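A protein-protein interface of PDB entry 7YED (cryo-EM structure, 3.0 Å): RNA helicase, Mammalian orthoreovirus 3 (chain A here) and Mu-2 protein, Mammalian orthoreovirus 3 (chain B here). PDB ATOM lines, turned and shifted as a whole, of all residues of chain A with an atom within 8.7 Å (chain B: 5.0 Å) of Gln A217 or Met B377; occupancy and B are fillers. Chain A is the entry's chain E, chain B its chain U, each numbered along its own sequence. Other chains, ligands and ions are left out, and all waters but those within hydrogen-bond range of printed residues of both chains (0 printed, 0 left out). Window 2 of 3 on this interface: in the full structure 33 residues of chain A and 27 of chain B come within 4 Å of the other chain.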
ATOM      1  N   SER A 213     -20.171  11.703 -17.211  1.00  0.00           N
ATOM      2  CA  SER A 213     -21.303  12.207 -16.443  1.00  0.00           C
ATOM      3  C   SER A 213     -20.868  12.804 -15.116  1.00  0.00           C
ATOM      4  O   SER A 213     -21.605  13.594 -14.518  1.00  0.00           O
ATOM      5  CB  SER A 213     -22.318  11.099 -16.191  1.00  0.00           C
ATOM      6  OG  SER A 213     -23.386  11.575 -15.389  1.00  0.00           O
ATOM      7  N   SER A 214     -19.669  12.411 -14.664  1.00  0.00           N
ATOM      8  CA  SER A 214     -19.159  12.876 -13.377  1.00  0.00           C
ATOM      9  C   SER A 214     -19.115  14.394 -13.315  1.00  0.00           C
ATOM     10  O   SER A 214     -19.349  14.980 -12.253  1.00  0.00           O
ATOM     11  CB  SER A 214     -17.773  12.285 -13.115  1.00  0.00           C
ATOM     12  OG  SER A 214     -17.248  12.736 -11.879  1.00  0.00           O
ATOM     13  N   GLU A 215     -18.849  15.044 -14.447  1.00  0.00           N
ATOM     14  CA  GLU A 215     -19.009  16.489 -14.528  1.00  0.00           C
ATOM     15  C   GLU A 215     -20.449  16.897 -14.219  1.00  0.00           C
ATOM     16  O   GLU A 215     -20.690  17.910 -13.547  1.00  0.00           O
ATOM     17  CB  GLU A 215     -18.585  16.964 -15.916  1.00  0.00           C
ATOM     18  CG  GLU A 215     -18.625  18.456 -16.127  1.00  0.00           C
ATOM     19  CD  GLU A 215     -17.651  19.189 -15.239  1.00  0.00           C
ATOM     20  OE1 GLU A 215     -16.647  18.574 -14.825  1.00  0.00           O
ATOM     21  OE2 GLU A 215     -17.887  20.381 -14.953  1.00  0.00           O
ATOM     22  N   ILE A 216     -21.419  16.099 -14.669  1.00  0.00           N
ATOM     23  CA  ILE A 216     -22.819  16.437 -14.431  1.00  0.00           C
ATOM     24  C   ILE A 216     -23.162  16.298 -12.954  1.00  0.00           C
ATOM     25  O   ILE A 216     -23.874  17.135 -12.383  1.00  0.00           O
ATOM     26  CB  ILE A 216     -23.735  15.567 -15.307  1.00  0.00           C
ATOM     27  CG1 ILE A 216     -23.422  15.789 -16.786  1.00  0.00           C
ATOM     28  CG2 ILE A 216     -25.188  15.878 -15.019  1.00  0.00           C
ATOM     29  CD1 ILE A 216     -23.635  17.215 -17.242  1.00  0.00           C
ATOM     30  N   GLN A 217     -22.672  15.235 -12.312  1.00  0.00           N
ATOM     31  CA  GLN A 217     -22.913  15.101 -10.879  1.00  0.00           C
ATOM     32  C   GLN A 217     -22.180  16.177 -10.086  1.00  0.00           C
ATOM     33  O   GLN A 217     -22.663  16.605  -9.030  1.00  0.00           O
ATOM     34  CB  GLN A 217     -22.535  13.701 -10.387  1.00  0.00           C
ATOM     35  CG  GLN A 217     -23.489  12.607 -10.865  1.00  0.00           C
ATOM     36  CD  GLN A 217     -23.041  11.987 -12.155  1.00  0.00           C
ATOM     37  OE1 GLN A 217     -21.858  12.024 -12.484  1.00  0.00           O
ATOM     38  NE2 GLN A 217     -23.978  11.432 -12.915  1.00  0.00           N
ATOM     39  N   ARG A 218     -21.025  16.633 -10.575  1.00  0.00           N
ATOM     40  CA  ARG A 218     -20.384  17.802  -9.984  1.00  0.00           C
ATOM     41  C   ARG A 218     -21.303  19.014 -10.054  1.00  0.00           C
ATOM     42  O   ARG A 218     -21.439  19.763  -9.079  1.00  0.00           O
ATOM     43  CB  ARG A 218     -19.059  18.087 -10.688  1.00  0.00           C
ATOM     44  CG  ARG A 218     -18.012  17.011 -10.479  1.00  0.00           C
ATOM     45  CD  ARG A 218     -16.731  17.327 -11.226  1.00  0.00           C
ATOM     46  NE  ARG A 218     -16.065  18.507 -10.685  1.00  0.00           N
ATOM     47  CZ  ARG A 218     -15.017  19.096 -11.250  1.00  0.00           C
ATOM     48  NH1 ARG A 218     -14.511  18.616 -12.378  1.00  0.00           N
ATOM     49  NH2 ARG A 218     -14.473  20.167 -10.687  1.00  0.00           N
ATOM     50  N   HIS A 219     -21.937  19.227 -11.212  1.00  0.00           N
ATOM     51  CA  HIS A 219     -22.931  20.292 -11.330  1.00  0.00           C
ATOM     52  C   HIS A 219     -24.048  20.130 -10.304  1.00  0.00           C
ATOM     53  O   HIS A 219     -24.479  21.109  -9.680  1.00  0.00           O
ATOM     54  CB  HIS A 219     -23.527  20.317 -12.735  1.00  0.00           C
ATOM     55  CG  HIS A 219     -22.566  20.733 -13.801  1.00  0.00           C
ATOM     56  ND1 HIS A 219     -21.794  19.833 -14.502  1.00  0.00           N
ATOM     57  CD2 HIS A 219     -22.259  21.956 -14.293  1.00  0.00           C
ATOM     58  CE1 HIS A 219     -21.054  20.483 -15.380  1.00  0.00           C
ATOM     59  NE2 HIS A 219     -21.314  21.774 -15.271  1.00  0.00           N
ATOM     60  N   ILE A 220     -24.534  18.903 -10.130  1.00  0.00           N
ATOM     61  CA  ILE A 220     -25.640  18.665  -9.201  1.00  0.00           C
ATOM     62  C   ILE A 220     -25.226  19.024  -7.779  1.00  0.00           C
ATOM     63  O   ILE A 220     -25.962  19.701  -7.046  1.00  0.00           O
ATOM     64  CB  ILE A 220     -26.118  17.206  -9.292  1.00  0.00           C
ATOM     65  CG1 ILE A 220     -26.669  16.914 -10.685  1.00  0.00           C
ATOM     66  CG2 ILE A 220     -27.173  16.930  -8.236  1.00  0.00           C
ATOM     67  CD1 ILE A 220     -26.912  15.449 -10.942  1.00  0.00           C
ATOM     68  N   THR A 221     -24.044  18.568  -7.366  1.00  0.00           N
ATOM     69  CA  THR A 221     -23.580  18.861  -6.015  1.00  0.00           C
ATOM     70  C   THR A 221     -23.356  20.353  -5.823  1.00  0.00           C
ATOM     71  O   THR A 221     -23.662  20.902  -4.756  1.00  0.00           O
ATOM     72  CB  THR A 221     -22.301  18.086  -5.714  1.00  0.00           C
ATOM     73  OG1 THR A 221     -22.556  16.683  -5.820  1.00  0.00           O
ATOM     74  CG2 THR A 221     -21.819  18.400  -4.312  1.00  0.00           C
ATOM     75  N   GLU A 222     -22.838  21.032  -6.849  1.00  0.00           N
ATOM     76  CA  GLU A 222     -22.639  22.472  -6.741  1.00  0.00           C
ATOM     77  C   GLU A 222     -23.968  23.196  -6.591  1.00  0.00           C
ATOM     78  O   GLU A 222     -24.080  24.142  -5.800  1.00  0.00           O
ATOM     79  CB  GLU A 222     -21.872  22.992  -7.954  1.00  0.00           C
ATOM     80  CG  GLU A 222     -20.439  22.496  -8.020  1.00  0.00           C
ATOM     81  CD  GLU A 222     -19.697  23.005  -9.236  1.00  0.00           C
ATOM     82  OE1 GLU A 222     -20.329  23.664 -10.084  1.00  0.00           O
ATOM     83  OE2 GLU A 222     -18.483  22.741  -9.352  1.00  0.00           O
ATOM     84  N   PHE A 223     -24.998  22.755  -7.316  1.00  0.00           N
ATOM     85  CA  PHE A 223     -26.285  23.423  -7.171  1.00  0.00           C
ATOM     86  C   PHE A 223     -26.894  23.162  -5.804  1.00  0.00           C
ATOM     87  O   PHE A 223     -27.508  24.057  -5.218  1.00  0.00           O
ATOM     88  CB  PHE A 223     -27.269  23.010  -8.258  1.00  0.00           C
ATOM     89  CG  PHE A 223     -28.605  23.679  -8.113  1.00  0.00           C
ATOM     90  CD1 PHE A 223     -28.730  25.039  -8.339  1.00  0.00           C
ATOM     91  CD2 PHE A 223     -29.724  22.967  -7.721  1.00  0.00           C
ATOM     92  CE1 PHE A 223     -29.946  25.670  -8.201  1.00  0.00           C
ATOM     93  CE2 PHE A 223     -30.947  23.596  -7.577  1.00  0.00           C
ATOM     94  CZ  PHE A 223     -31.056  24.947  -7.818  1.00  0.00           C
ATOM     95  N   ILE A 224     -26.744  21.947  -5.277  1.00  0.00           N
ATOM     96  CA  ILE A 224     -27.311  21.681  -3.961  1.00  0.00           C
ATOM     97  C   ILE A 224     -26.596  22.502  -2.896  1.00  0.00           C
ATOM     98  O   ILE A 224     -27.221  23.013  -1.957  1.00  0.00           O
ATOM     99  CB  ILE A 224     -27.271  20.177  -3.645  1.00  0.00           C
ATOM    100  CG1 ILE A 224     -28.112  19.410  -4.661  1.00  0.00           C
ATOM    101  CG2 ILE A 224     -27.805  19.927  -2.254  1.00  0.00           C
ATOM    102  CD1 ILE A 224     -27.952  17.921  -4.574  1.00  0.00           C
ATOM    103  N   SER A 225     -25.280  22.675  -3.037  1.00  0.00           N
ATOM    104  CA  SER A 225     -24.549  23.520  -2.098  1.00  0.00           C
ATOM    105  C   SER A 225     -25.017  24.969  -2.184  1.00  0.00           C
ATOM    106  O   SER A 225     -25.272  25.618  -1.160  1.00  0.00           O
ATOM    107  CB  SER A 225     -23.051  23.418  -2.371  1.00  0.00           C
ATOM    108  OG  SER A 225     -22.591  22.097  -2.166  1.00  0.00           O
ATOM    109  N   GLN A 228     -28.233  25.335  -0.467  1.00  0.00           N
ATOM    110  CA  GLN A 228     -28.093  25.361   0.984  1.00  0.00           C
ATOM    111  C   GLN A 228     -27.527  26.681   1.484  1.00  0.00           C
ATOM    112  O   GLN A 228     -27.710  27.016   2.658  1.00  0.00           O
ATOM    113  CB  GLN A 228     -27.201  24.212   1.451  1.00  0.00           C
ATOM    114  CG  GLN A 228     -27.761  22.838   1.162  1.00  0.00           C
ATOM    115  CD  GLN A 228     -29.026  22.557   1.937  1.00  0.00           C
ATOM    116  OE1 GLN A 228     -29.152  22.941   3.099  1.00  0.00           O
ATOM    117  NE2 GLN A 228     -29.973  21.882   1.298  1.00  0.00           N
ATOM    118  N   ASN B 373     -34.217  17.195   0.678  1.00  0.00           N
ATOM    119  CA  ASN B 373     -33.567  16.863  -0.588  1.00  0.00           C
ATOM    120  C   ASN B 373     -34.188  15.610  -1.197  1.00  0.00           C
ATOM    121  O   ASN B 373     -34.307  14.594  -0.512  1.00  0.00           O
ATOM    122  CB  ASN B 373     -32.074  16.652  -0.355  1.00  0.00           C
ATOM    123  CG  ASN B 373     -31.291  16.487  -1.637  1.00  0.00           C
ATOM    124  OD1 ASN B 373     -31.848  16.511  -2.728  1.00  0.00           O
ATOM    125  ND2 ASN B 373     -29.983  16.313  -1.508  1.00  0.00           N
ATOM    126  N   SER B 375     -32.916  13.889  -3.869  1.00  0.00           N
ATOM    127  CA  SER B 375     -31.904  13.035  -4.472  1.00  0.00           C
ATOM    128  C   SER B 375     -31.292  12.121  -3.418  1.00  0.00           C
ATOM    129  O   SER B 375     -31.801  11.978  -2.305  1.00  0.00           O
ATOM    130  CB  SER B 375     -30.833  13.879  -5.154  1.00  0.00           C
ATOM    131  OG  SER B 375     -29.804  13.052  -5.663  1.00  0.00           O
ATOM    132  N   SER B 376     -30.184  11.477  -3.779  1.00  0.00           N
ATOM    133  CA  SER B 376     -29.406  10.665  -2.854  1.00  0.00           C
ATOM    134  C   SER B 376     -27.930  11.029  -2.937  1.00  0.00           C
ATOM    135  O   SER B 376     -27.061  10.197  -2.673  1.00  0.00           O
ATOM    136  CB  SER B 376     -29.615   9.175  -3.126  1.00  0.00           C
ATOM    137  OG  SER B 376     -29.114   8.811  -4.400  1.00  0.00           O
ATOM    138  N   MET B 377     -27.658  12.288  -3.276  1.00  0.00           N
ATOM    139  CA  MET B 377     -26.280  12.764  -3.378  1.00  0.00           C
ATOM    140  C   MET B 377     -26.012  13.857  -2.352  1.00  0.00           C
ATOM    141  O   MET B 377     -26.850  14.737  -2.152  1.00  0.00           O
ATOM    142  CB  MET B 377     -26.020  13.315  -4.779  1.00  0.00           C
ATOM    143  CG  MET B 377     -26.147  12.292  -5.894  1.00  0.00           C
ATOM    144  SD  MET B 377     -25.917  13.065  -7.503  1.00  0.00           S
ATOM    145  CE  MET B 377     -24.469  14.061  -7.165  1.00  0.00           C
ATOM    146  N   PRO B 378     -24.837  13.823  -1.708  1.00  0.00           N
ATOM    147  CA  PRO B 378     -24.469  14.830  -0.701  1.00  0.00           C
ATOM    148  C   PRO B 378     -24.169  16.189  -1.342  1.00  0.00           C
ATOM    149  O   PRO B 378     -23.967  16.237  -2.555  1.00  0.00           O
ATOM    150  CB  PRO B 378     -23.204  14.238  -0.071  1.00  0.00           C
ATOM    151  CG  PRO B 378     -22.636  13.344  -1.120  1.00  0.00           C
ATOM    152  CD  PRO B 378     -23.824  12.759  -1.824  1.00  0.00           C
ATOM    153  N   PRO B 379     -24.174  17.292  -0.566  1.00  0.00           N
ATOM    154  CA  PRO B 379     -24.067  17.527   0.887  1.00  0.00           C
ATOM    155  C   PRO B 379     -25.179  17.033   1.820  1.00  0.00           C
ATOM    156  O   PRO B 379     -24.851  16.507   2.882  1.00  0.00           O
ATOM    157  CB  PRO B 379     -23.947  19.056   0.990  1.00  0.00           C
ATOM    158  CG  PRO B 379     -24.572  19.571  -0.256  1.00  0.00           C
ATOM    159  CD  PRO B 379     -24.241  18.561  -1.312  1.00  0.00           C
ATOM    160  N   ASP B 380     -26.449  17.183   1.453  1.00  0.00           N
ATOM    161  CA  ASP B 380     -27.534  16.824   2.377  1.00  0.00           C
ATOM    162  C   ASP B 380     -28.409  15.668   1.926  1.00  0.00           C
ATOM    163  O   ASP B 380     -29.064  15.762   0.898  1.00  0.00           O
ATOM    164  CB  ASP B 380     -28.404  18.047   2.676  1.00  0.00           C
ATOM    165  CG  ASP B 380     -27.739  19.016   3.631  1.00  0.00           C
ATOM    166  OD1 ASP B 380     -26.693  18.664   4.214  1.00  0.00           O
ATOM    167  OD2 ASP B 380     -28.269  20.127   3.811  1.00  0.00           O
ATOM    168  N   VAL B 381     -28.436  14.585   2.699  1.00  0.00           N
ATOM    169  CA  VAL B 381     -29.228  13.411   2.357  1.00  0.00           C
ATOM    170  C   VAL B 381     -29.899  12.915   3.626  1.00  0.00           C
ATOM    171  O   VAL B 381     -29.226  12.639   4.625  1.00  0.00           O
ATOM    172  CB  VAL B 381     -28.363  12.304   1.729  1.00  0.00           C
ATOM    173  CG1 VAL B 381     -29.195  11.063   1.497  1.00  0.00           C
ATOM    174  CG2 VAL B 381     -27.748  12.779   0.431  1.00  0.00           C
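The side-chain amide oxygen (OE1) of Gln A228 sits close to the side-chain carboxylate (OD2) of Asp B380, 3.0 Å away.
The side-chain hydroxyl (OG) of Ser A213 sits at hydrogen-bond distance from the side-chain amide nitrogen (NE2) of Gln A217 (2.5 Å).
OE1 of Gln A217 sits close to N of Ser A214, at 3.1 Å.
OG1 of Thr A221 lies within hydrogen-bond range of O of Gln A217.
O of Thr A221 is in hydrogen-bond range of OG of Ser A225 (3.0 Å).
O of Asp B380 lies within hydrogen-bond range of ND2 of Asn B373 (2.6 Å).
The side-chain hydroxyl of Ser B375 sits at hydrogen-bond distance from the backbone NH of Met B377.
Among the printed residues, pairs that only touch across the chains: Gln A217 with Met B377, Thr A221 with Met B377, Thr A221 with Pro B378, Thr A221 with Pro B379, Ile A224 with Pro B379 and Ser A225 with Pro B379.
Of chain B, only Met B377 (3.6 Å) comes within 4 Å of Gln A217.
Of the printed residues of chain B, Thr A221 touches Met B377 (3.5 Å), Pro B378 (3.5 Å) and Pro B379 (3.9 Å).
Of the printed residues of chain B, Ile A224 touches Pro B379.
Of the printed residues of chain B, Gln A228 touches Asp B380.
No residue of chain A comes within 4 Å of Ser B376.
Of the printed residues of chain A, Met B377 touches Gln A217 (3.6 Å) and Thr A221 (3.5 Å).
Pro B378 touches just one residue of chain A: Thr A221.
Of the printed residues of chain A, Asp B380 touches Gln A228 (3.0 Å).
The nearest printed residue of chain B that does not touch Gln A217 is Pro B378 (6.6 Å).
Of the 14 printed residues of chain A, 5 touch a printed residue of chain B.
Hydrophobic or aromatic side chains of chain B within 4 Å of the printed part of chain A: Met B377 and Pro B379.
Among the printed residues, 7 pairs touch across the chains.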
